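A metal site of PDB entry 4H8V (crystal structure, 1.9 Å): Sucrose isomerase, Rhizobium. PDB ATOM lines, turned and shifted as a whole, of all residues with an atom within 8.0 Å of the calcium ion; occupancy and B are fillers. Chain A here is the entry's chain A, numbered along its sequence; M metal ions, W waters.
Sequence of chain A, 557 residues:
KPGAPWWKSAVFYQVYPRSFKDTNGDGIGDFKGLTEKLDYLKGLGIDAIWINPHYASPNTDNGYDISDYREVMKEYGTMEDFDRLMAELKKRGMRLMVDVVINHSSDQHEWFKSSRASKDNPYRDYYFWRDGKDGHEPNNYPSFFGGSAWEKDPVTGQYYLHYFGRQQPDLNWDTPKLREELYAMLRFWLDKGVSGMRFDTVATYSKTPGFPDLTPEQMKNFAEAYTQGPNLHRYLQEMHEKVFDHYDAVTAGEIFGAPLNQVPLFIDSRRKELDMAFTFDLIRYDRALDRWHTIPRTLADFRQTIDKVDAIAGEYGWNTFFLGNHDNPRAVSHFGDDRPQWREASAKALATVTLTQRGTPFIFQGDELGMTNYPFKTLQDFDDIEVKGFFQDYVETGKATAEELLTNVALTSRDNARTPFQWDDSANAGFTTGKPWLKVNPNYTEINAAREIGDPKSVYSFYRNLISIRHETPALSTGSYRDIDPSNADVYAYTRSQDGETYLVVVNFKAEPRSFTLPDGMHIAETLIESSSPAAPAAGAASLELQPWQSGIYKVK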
ATOM      1  N   PRO A  17      -6.268 -13.885   2.366  1.00  0.00           N
ATOM      2  CA  PRO A  17      -7.214 -13.901   1.225  1.00  0.00           C
ATOM      3  C   PRO A  17      -6.754 -13.153  -0.023  1.00  0.00           C
ATOM      4  O   PRO A  17      -7.176 -13.498  -1.128  1.00  0.00           O
ATOM      5  CB  PRO A  17      -8.489 -13.275   1.796  1.00  0.00           C
ATOM      6  CG  PRO A  17      -8.124 -12.715   3.112  1.00  0.00           C
ATOM      7  CD  PRO A  17      -6.913 -13.416   3.602  1.00  0.00           C
ATOM      8  N   ARG A  18      -5.894 -12.162   0.161  1.00  0.00           N
ATOM      9  CA  ARG A  18      -5.345 -11.399  -0.930  1.00  0.00           C
ATOM     10  C   ARG A  18      -4.583 -12.315  -1.892  1.00  0.00           C
ATOM     11  O   ARG A  18      -4.546 -12.066  -3.103  1.00  0.00           O
ATOM     12  CB  ARG A  18      -4.409 -10.322  -0.364  1.00  0.00           C
ATOM     13  CG  ARG A  18      -3.960  -9.285  -1.351  1.00  0.00           C
ATOM     14  CD  ARG A  18      -3.014  -8.272  -0.719  1.00  0.00           C
ATOM     15  NE  ARG A  18      -2.518  -7.357  -1.749  1.00  0.00           N
ATOM     16  CZ  ARG A  18      -3.155  -6.252  -2.129  1.00  0.00           C
ATOM     17  NH1 ARG A  18      -4.299  -5.906  -1.521  1.00  0.00           N
ATOM     18  NH2 ARG A  18      -2.646  -5.483  -3.074  1.00  0.00           N
ATOM     19  N   LYS A  21      -7.179 -17.122  -3.611  1.00  0.00           N
ATOM     20  CA  LYS A  21      -7.826 -17.367  -4.900  1.00  0.00           C
ATOM     21  C   LYS A  21      -8.559 -16.136  -5.441  1.00  0.00           C
ATOM     22  O   LYS A  21      -9.422 -15.574  -4.763  1.00  0.00           O
ATOM     23  CB  LYS A  21      -8.787 -18.550  -4.832  1.00  0.00           C
ATOM     24  CG  LYS A  21      -9.430 -18.917  -6.165  1.00  0.00           C
ATOM     25  CD  LYS A  21      -8.383 -19.345  -7.201  1.00  0.00           C
ATOM     26  CE  LYS A  21      -8.989 -20.198  -8.289  1.00  0.00           C
ATOM     27  NZ  LYS A  21     -10.204 -19.600  -8.883  1.00  0.00           N
ATOM     28  N   ASP A  22      -8.205 -15.745  -6.665  1.00  0.00           N
ATOM     29  CA  ASP A  22      -8.856 -14.628  -7.349  1.00  0.00           C
ATOM     30  C   ASP A  22      -9.918 -15.201  -8.285  1.00  0.00           C
ATOM     31  O   ASP A  22      -9.666 -16.171  -8.993  1.00  0.00           O
ATOM     32  CB  ASP A  22      -7.805 -13.817  -8.124  1.00  0.00           C
ATOM     33  CG  ASP A  22      -8.397 -12.657  -8.921  1.00  0.00           C
ATOM     34  OD1 ASP A  22      -9.548 -12.265  -8.654  1.00  0.00           O
ATOM     35  OD2 ASP A  22      -7.715 -12.129  -9.826  1.00  0.00           O
ATOM     36  N   THR A  23     -11.114 -14.612  -8.286  1.00  0.00           N
ATOM     37  CA  THR A  23     -12.172 -15.103  -9.167  1.00  0.00           C
ATOM     38  C   THR A  23     -12.708 -14.041 -10.110  1.00  0.00           C
ATOM     39  O   THR A  23     -13.727 -14.263 -10.766  1.00  0.00           O
ATOM     40  CB  THR A  23     -13.374 -15.667  -8.404  1.00  0.00           C
ATOM     41  OG1 THR A  23     -13.886 -14.677  -7.515  1.00  0.00           O
ATOM     42  CG2 THR A  23     -12.979 -16.892  -7.611  1.00  0.00           C
ATOM     43  N   ASN A  24     -12.052 -12.891 -10.177  1.00  0.00           N
ATOM     44  CA  ASN A  24     -12.468 -11.873 -11.143  1.00  0.00           C
ATOM     45  C   ASN A  24     -11.300 -11.272 -11.931  1.00  0.00           C
ATOM     46  O   ASN A  24     -11.439 -10.203 -12.541  1.00  0.00           O
ATOM     47  CB  ASN A  24     -13.285 -10.770 -10.468  1.00  0.00           C
ATOM     48  CG  ASN A  24     -12.458  -9.910  -9.545  1.00  0.00           C
ATOM     49  OD1 ASN A  24     -11.440 -10.352  -9.026  1.00  0.00           O
ATOM     50  ND2 ASN A  24     -12.896  -8.680  -9.333  1.00  0.00           N
ATOM     51  N   GLY A  25     -10.151 -11.954 -11.910  1.00  0.00           N
ATOM     52  CA  GLY A  25      -9.013 -11.578 -12.739  1.00  0.00           C
ATOM     53  C   GLY A  25      -8.302 -10.257 -12.429  1.00  0.00           C
ATOM     54  O   GLY A  25      -7.437  -9.819 -13.205  1.00  0.00           O
ATOM     55  N   ASP A  26      -8.636  -9.631 -11.303  1.00  0.00           N
ATOM     56  CA  ASP A  26      -8.007  -8.354 -10.977  1.00  0.00           C
ATOM     57  C   ASP A  26      -6.658  -8.580 -10.314  1.00  0.00           C
ATOM     58  O   ASP A  26      -5.945  -7.630 -10.019  1.00  0.00           O
ATOM     59  CB  ASP A  26      -8.924  -7.477 -10.119  1.00  0.00           C
ATOM     60  CG  ASP A  26      -9.142  -8.019  -8.713  1.00  0.00           C
ATOM     61  OD1 ASP A  26      -8.798  -9.186  -8.458  1.00  0.00           O
ATOM     62  OD2 ASP A  26      -9.658  -7.265  -7.871  1.00  0.00           O
ATOM     63  N   GLY A  27      -6.305  -9.843 -10.085  1.00  0.00           N
ATOM     64  CA  GLY A  27      -5.004 -10.185  -9.547  1.00  0.00           C
ATOM     65  C   GLY A  27      -4.948 -10.289  -8.034  1.00  0.00           C
ATOM     66  O   GLY A  27      -3.893 -10.595  -7.471  1.00  0.00           O
ATOM     67  N   ILE A  28      -6.077 -10.014  -7.376  1.00  0.00           N
ATOM     68  CA  ILE A  28      -6.184 -10.049  -5.920  1.00  0.00           C
ATOM     69  C   ILE A  28      -7.215 -11.114  -5.526  1.00  0.00           C
ATOM     70  O   ILE A  28      -8.296 -11.190  -6.101  1.00  0.00           O
ATOM     71  CB  ILE A  28      -6.633  -8.674  -5.373  1.00  0.00           C
ATOM     72  CG1 ILE A  28      -5.565  -7.610  -5.659  1.00  0.00           C
ATOM     73  CG2 ILE A  28      -6.958  -8.770  -3.871  1.00  0.00           C
ATOM     74  CD1 ILE A  28      -6.036  -6.169  -5.549  1.00  0.00           C
ATOM     75  N   GLY A  29      -6.867 -11.952  -4.565  1.00  0.00           N
ATOM     76  CA  GLY A  29      -7.791 -12.995  -4.139  1.00  0.00           C
ATOM     77  C   GLY A  29      -9.005 -12.409  -3.425  1.00  0.00           C
ATOM     78  O   GLY A  29      -8.936 -11.301  -2.888  1.00  0.00           O
ATOM     79  N   ASP A  30     -10.107 -13.137  -3.423  1.00  0.00           N
ATOM     80  CA  ASP A  30     -11.344 -12.621  -2.863  1.00  0.00           C
ATOM     81  C   ASP A  30     -12.113 -13.693  -2.116  1.00  0.00           C
ATOM     82  O   ASP A  30     -11.717 -14.856  -2.071  1.00  0.00           O
ATOM     83  CB  ASP A  30     -12.221 -12.059  -3.981  1.00  0.00           C
ATOM     84  CG  ASP A  30     -12.132 -12.880  -5.257  1.00  0.00           C
ATOM     85  OD1 ASP A  30     -12.756 -13.960  -5.322  1.00  0.00           O
ATOM     86  OD2 ASP A  30     -11.438 -12.440  -6.182  1.00  0.00           O
ATOM     87  N   PHE A  31     -13.241 -13.274  -1.531  1.00  0.00           N
ATOM     88  CA  PHE A  31     -14.113 -14.188  -0.804  1.00  0.00           C
ATOM     89  C   PHE A  31     -14.653 -15.330  -1.647  1.00  0.00           C
ATOM     90  O   PHE A  31     -14.603 -16.474  -1.222  1.00  0.00           O
ATOM     91  CB  PHE A  31     -15.285 -13.431  -0.179  1.00  0.00           C
ATOM     92  CG  PHE A  31     -14.924 -12.756   1.092  1.00  0.00           C
ATOM     93  CD1 PHE A  31     -13.907 -13.270   1.876  1.00  0.00           C
ATOM     94  CD2 PHE A  31     -15.558 -11.615   1.489  1.00  0.00           C
ATOM     95  CE1 PHE A  31     -13.554 -12.664   3.055  1.00  0.00           C
ATOM     96  CE2 PHE A  31     -15.209 -10.992   2.667  1.00  0.00           C
ATOM     97  CZ  PHE A  31     -14.209 -11.522   3.451  1.00  0.00           C
ATOM     98  N   LYS A  32     -15.170 -15.012  -2.825  1.00  0.00           N
ATOM     99  CA  LYS A  32     -15.706 -16.049  -3.707  1.00  0.00           C
ATOM    100  C   LYS A  32     -14.635 -17.088  -4.007  1.00  0.00           C
ATOM    101  O   LYS A  32     -14.929 -18.276  -4.128  1.00  0.00           O
ATOM    102  CB  LYS A  32     -16.250 -15.442  -5.008  1.00  0.00           C
ATOM    103  CG  LYS A  32     -17.574 -14.729  -4.837  1.00  0.00           C
ATOM    104  CD  LYS A  32     -18.010 -14.078  -6.140  1.00  0.00           C
ATOM    105  CE  LYS A  32     -19.270 -13.230  -5.950  1.00  0.00           C
ATOM    106  NZ  LYS A  32     -19.584 -12.448  -7.174  1.00  0.00           N
ATOM    107  N   GLY A  33     -13.383 -16.647  -4.118  1.00  0.00           N
ATOM    108  CA  GLY A  33     -12.268 -17.548  -4.302  1.00  0.00           C
ATOM    109  C   GLY A  33     -12.090 -18.480  -3.134  1.00  0.00           C
ATOM    110  O   GLY A  33     -11.885 -19.680  -3.301  1.00  0.00           O
ATOM    111  N   LYS A  74     -13.405  -3.836  -0.283  1.00  0.00           N
ATOM    112  CA  LYS A  74     -13.997  -3.881  -1.618  1.00  0.00           C
ATOM    113  C   LYS A  74     -13.320  -4.920  -2.521  1.00  0.00           C
ATOM    114  O   LYS A  74     -13.973  -5.525  -3.376  1.00  0.00           O
ATOM    115  CB  LYS A  74     -13.940  -2.494  -2.274  1.00  0.00           C
ATOM    116  N   GLU A  75     -12.023  -5.132  -2.329  1.00  0.00           N
ATOM    117  CA  GLU A  75     -11.326  -6.141  -3.115  1.00  0.00           C
ATOM    118  C   GLU A  75     -11.797  -7.553  -2.828  1.00  0.00           C
ATOM    119  O   GLU A  75     -11.849  -8.385  -3.746  1.00  0.00           O
ATOM    120  CB  GLU A  75      -9.809  -6.036  -2.909  1.00  0.00           C
ATOM    121  CG  GLU A  75      -9.132  -4.905  -3.682  1.00  0.00           C
ATOM    122  CD  GLU A  75      -9.220  -3.562  -2.973  1.00  0.00           C
ATOM    123  OE1 GLU A  75      -9.859  -3.473  -1.901  1.00  0.00           O
ATOM    124  OE2 GLU A  75      -8.643  -2.588  -3.506  1.00  0.00           O
ATOM    125  N   TYR A  76     -12.167  -7.839  -1.584  1.00  0.00           N
ATOM    126  CA  TYR A  76     -12.529  -9.211  -1.195  1.00  0.00           C
ATOM    127  C   TYR A  76     -13.970  -9.564  -1.560  1.00  0.00           C
ATOM    128  O   TYR A  76     -14.294 -10.731  -1.705  1.00  0.00           O
ATOM    129  CB  TYR A  76     -12.261  -9.498   0.279  1.00  0.00           C
ATOM    130  CG  TYR A  76     -10.807  -9.342   0.684  1.00  0.00           C
ATOM    131  CD1 TYR A  76      -9.809  -9.259  -0.283  1.00  0.00           C
ATOM    132  CD2 TYR A  76     -10.429  -9.273   2.014  1.00  0.00           C
ATOM    133  CE1 TYR A  76      -8.488  -9.097   0.072  1.00  0.00           C
ATOM    134  CE2 TYR A  76      -9.112  -9.129   2.381  1.00  0.00           C
ATOM    135  CZ  TYR A  76      -8.137  -9.035   1.396  1.00  0.00           C
ATOM    136  OH  TYR A  76      -6.797  -8.856   1.750  1.00  0.00           O
ATOM    137  N   GLY A  77     -14.809  -8.546  -1.695  1.00  0.00           N
ATOM    138  CA  GLY A  77     -16.173  -8.719  -2.155  1.00  0.00           C
ATOM    139  C   GLY A  77     -17.176  -7.853  -1.403  1.00  0.00           C
ATOM    140  O   GLY A  77     -16.851  -6.730  -1.036  1.00  0.00           O
ATOM    141  N   PHE A 431      -4.074 -19.180  -9.742  1.00  0.00           N
ATOM    142  CA  PHE A 431      -4.521 -18.182  -8.784  1.00  0.00           C
ATOM    143  C   PHE A 431      -5.430 -17.111  -9.390  1.00  0.00           C
ATOM    144  O   PHE A 431      -6.393 -16.653  -8.749  1.00  0.00           O
ATOM    145  CB  PHE A 431      -3.317 -17.541  -8.074  1.00  0.00           C
ATOM    146  CG  PHE A 431      -3.640 -16.260  -7.344  1.00  0.00           C
ATOM    147  CD1 PHE A 431      -4.339 -16.283  -6.133  1.00  0.00           C
ATOM    148  CD2 PHE A 431      -3.242 -15.042  -7.856  1.00  0.00           C
ATOM    149  CE1 PHE A 431      -4.622 -15.115  -5.451  1.00  0.00           C
ATOM    150  CE2 PHE A 431      -3.520 -13.861  -7.178  1.00  0.00           C
ATOM    151  CZ  PHE A 431      -4.215 -13.896  -5.975  1.00  0.00           C
ATOM    152  N   THR A 432      -5.126 -16.702 -10.617  1.00  0.00           N
ATOM    153  CA  THR A 432      -5.872 -15.650 -11.300  1.00  0.00           C
ATOM    154  C   THR A 432      -5.808 -15.833 -12.816  1.00  0.00           C
ATOM    155  O   THR A 432      -4.882 -16.441 -13.342  1.00  0.00           O
ATOM    156  CB  THR A 432      -5.316 -14.249 -10.991  1.00  0.00           C
ATOM    157  OG1 THR A 432      -6.098 -13.272 -11.689  1.00  0.00           O
ATOM    158  CG2 THR A 432      -3.868 -14.140 -11.444  1.00  0.00           C
HETATM  159 CA    CA M   1     -10.273 -10.683  -7.134  1.00  0.00          CA
HETATM  160  O   HOH W   1     -10.214  -8.818  -5.754  1.00  0.00           O
HETATM  161  O   HOH W   2     -12.447  -9.859  -6.293  1.00  0.00           O
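The side-chain carboxylate of Asp 22 sits at hydrogen-bond distance from the backbone NH of Gly 25 (3.2 Å).
OD2 of Asp 22 is in hydrogen-bond range of N of Gly 27, at 2.7 Å.
The side-chain hydroxyl of Thr 432 lies within hydrogen-bond range of the side-chain carboxylate of Asp 22, at 2.7 Å.
O of Phe 431 lies within hydrogen-bond range of N of Asp 22 (2.9 Å).
The side-chain carboxylate of Asp 30 lies within hydrogen-bond range of the side-chain hydroxyl of Thr 23, at 2.6 Å.
The backbone NH (N) of Asp 30 is in hydrogen-bond range of the backbone carbonyl oxygen (O) of Lys 21, at 2.9 Å.
The side-chain carboxylate of Asp 30 sits at hydrogen-bond distance from the backbone NH of Gly 33, at 3.0 Å.
Within 4 Å of the calcium ion: Asp 22, Asn 24, Asp 26, Ile 28 and Asp 30.
The calcium ion is bound by the side-chain amide oxygen of Asn 24 (2.2 Å), the backbone carbonyl oxygen of Ile 28 (2.3 Å), the side-chain carboxylate of Asp 22 (2.3 Å), the side-chain carboxylate of Asp 30 (2.3 Å), water W1 (2.3 Å), water W2 (2.5 Å) and the side-chain carboxylate of Asp 26 (2.5 Å).
The calcium ion has seven donor atoms within binding distance.
Water W2 lies within hydrogen-bond range of O of Glu 75 (3.0 Å) and ND2 of Asn 24 (3.3 Å).
Water W1 lies within hydrogen-bond range of O of Glu 75 (2.6 Å) and OD2 of Asp 26 (2.7 Å).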
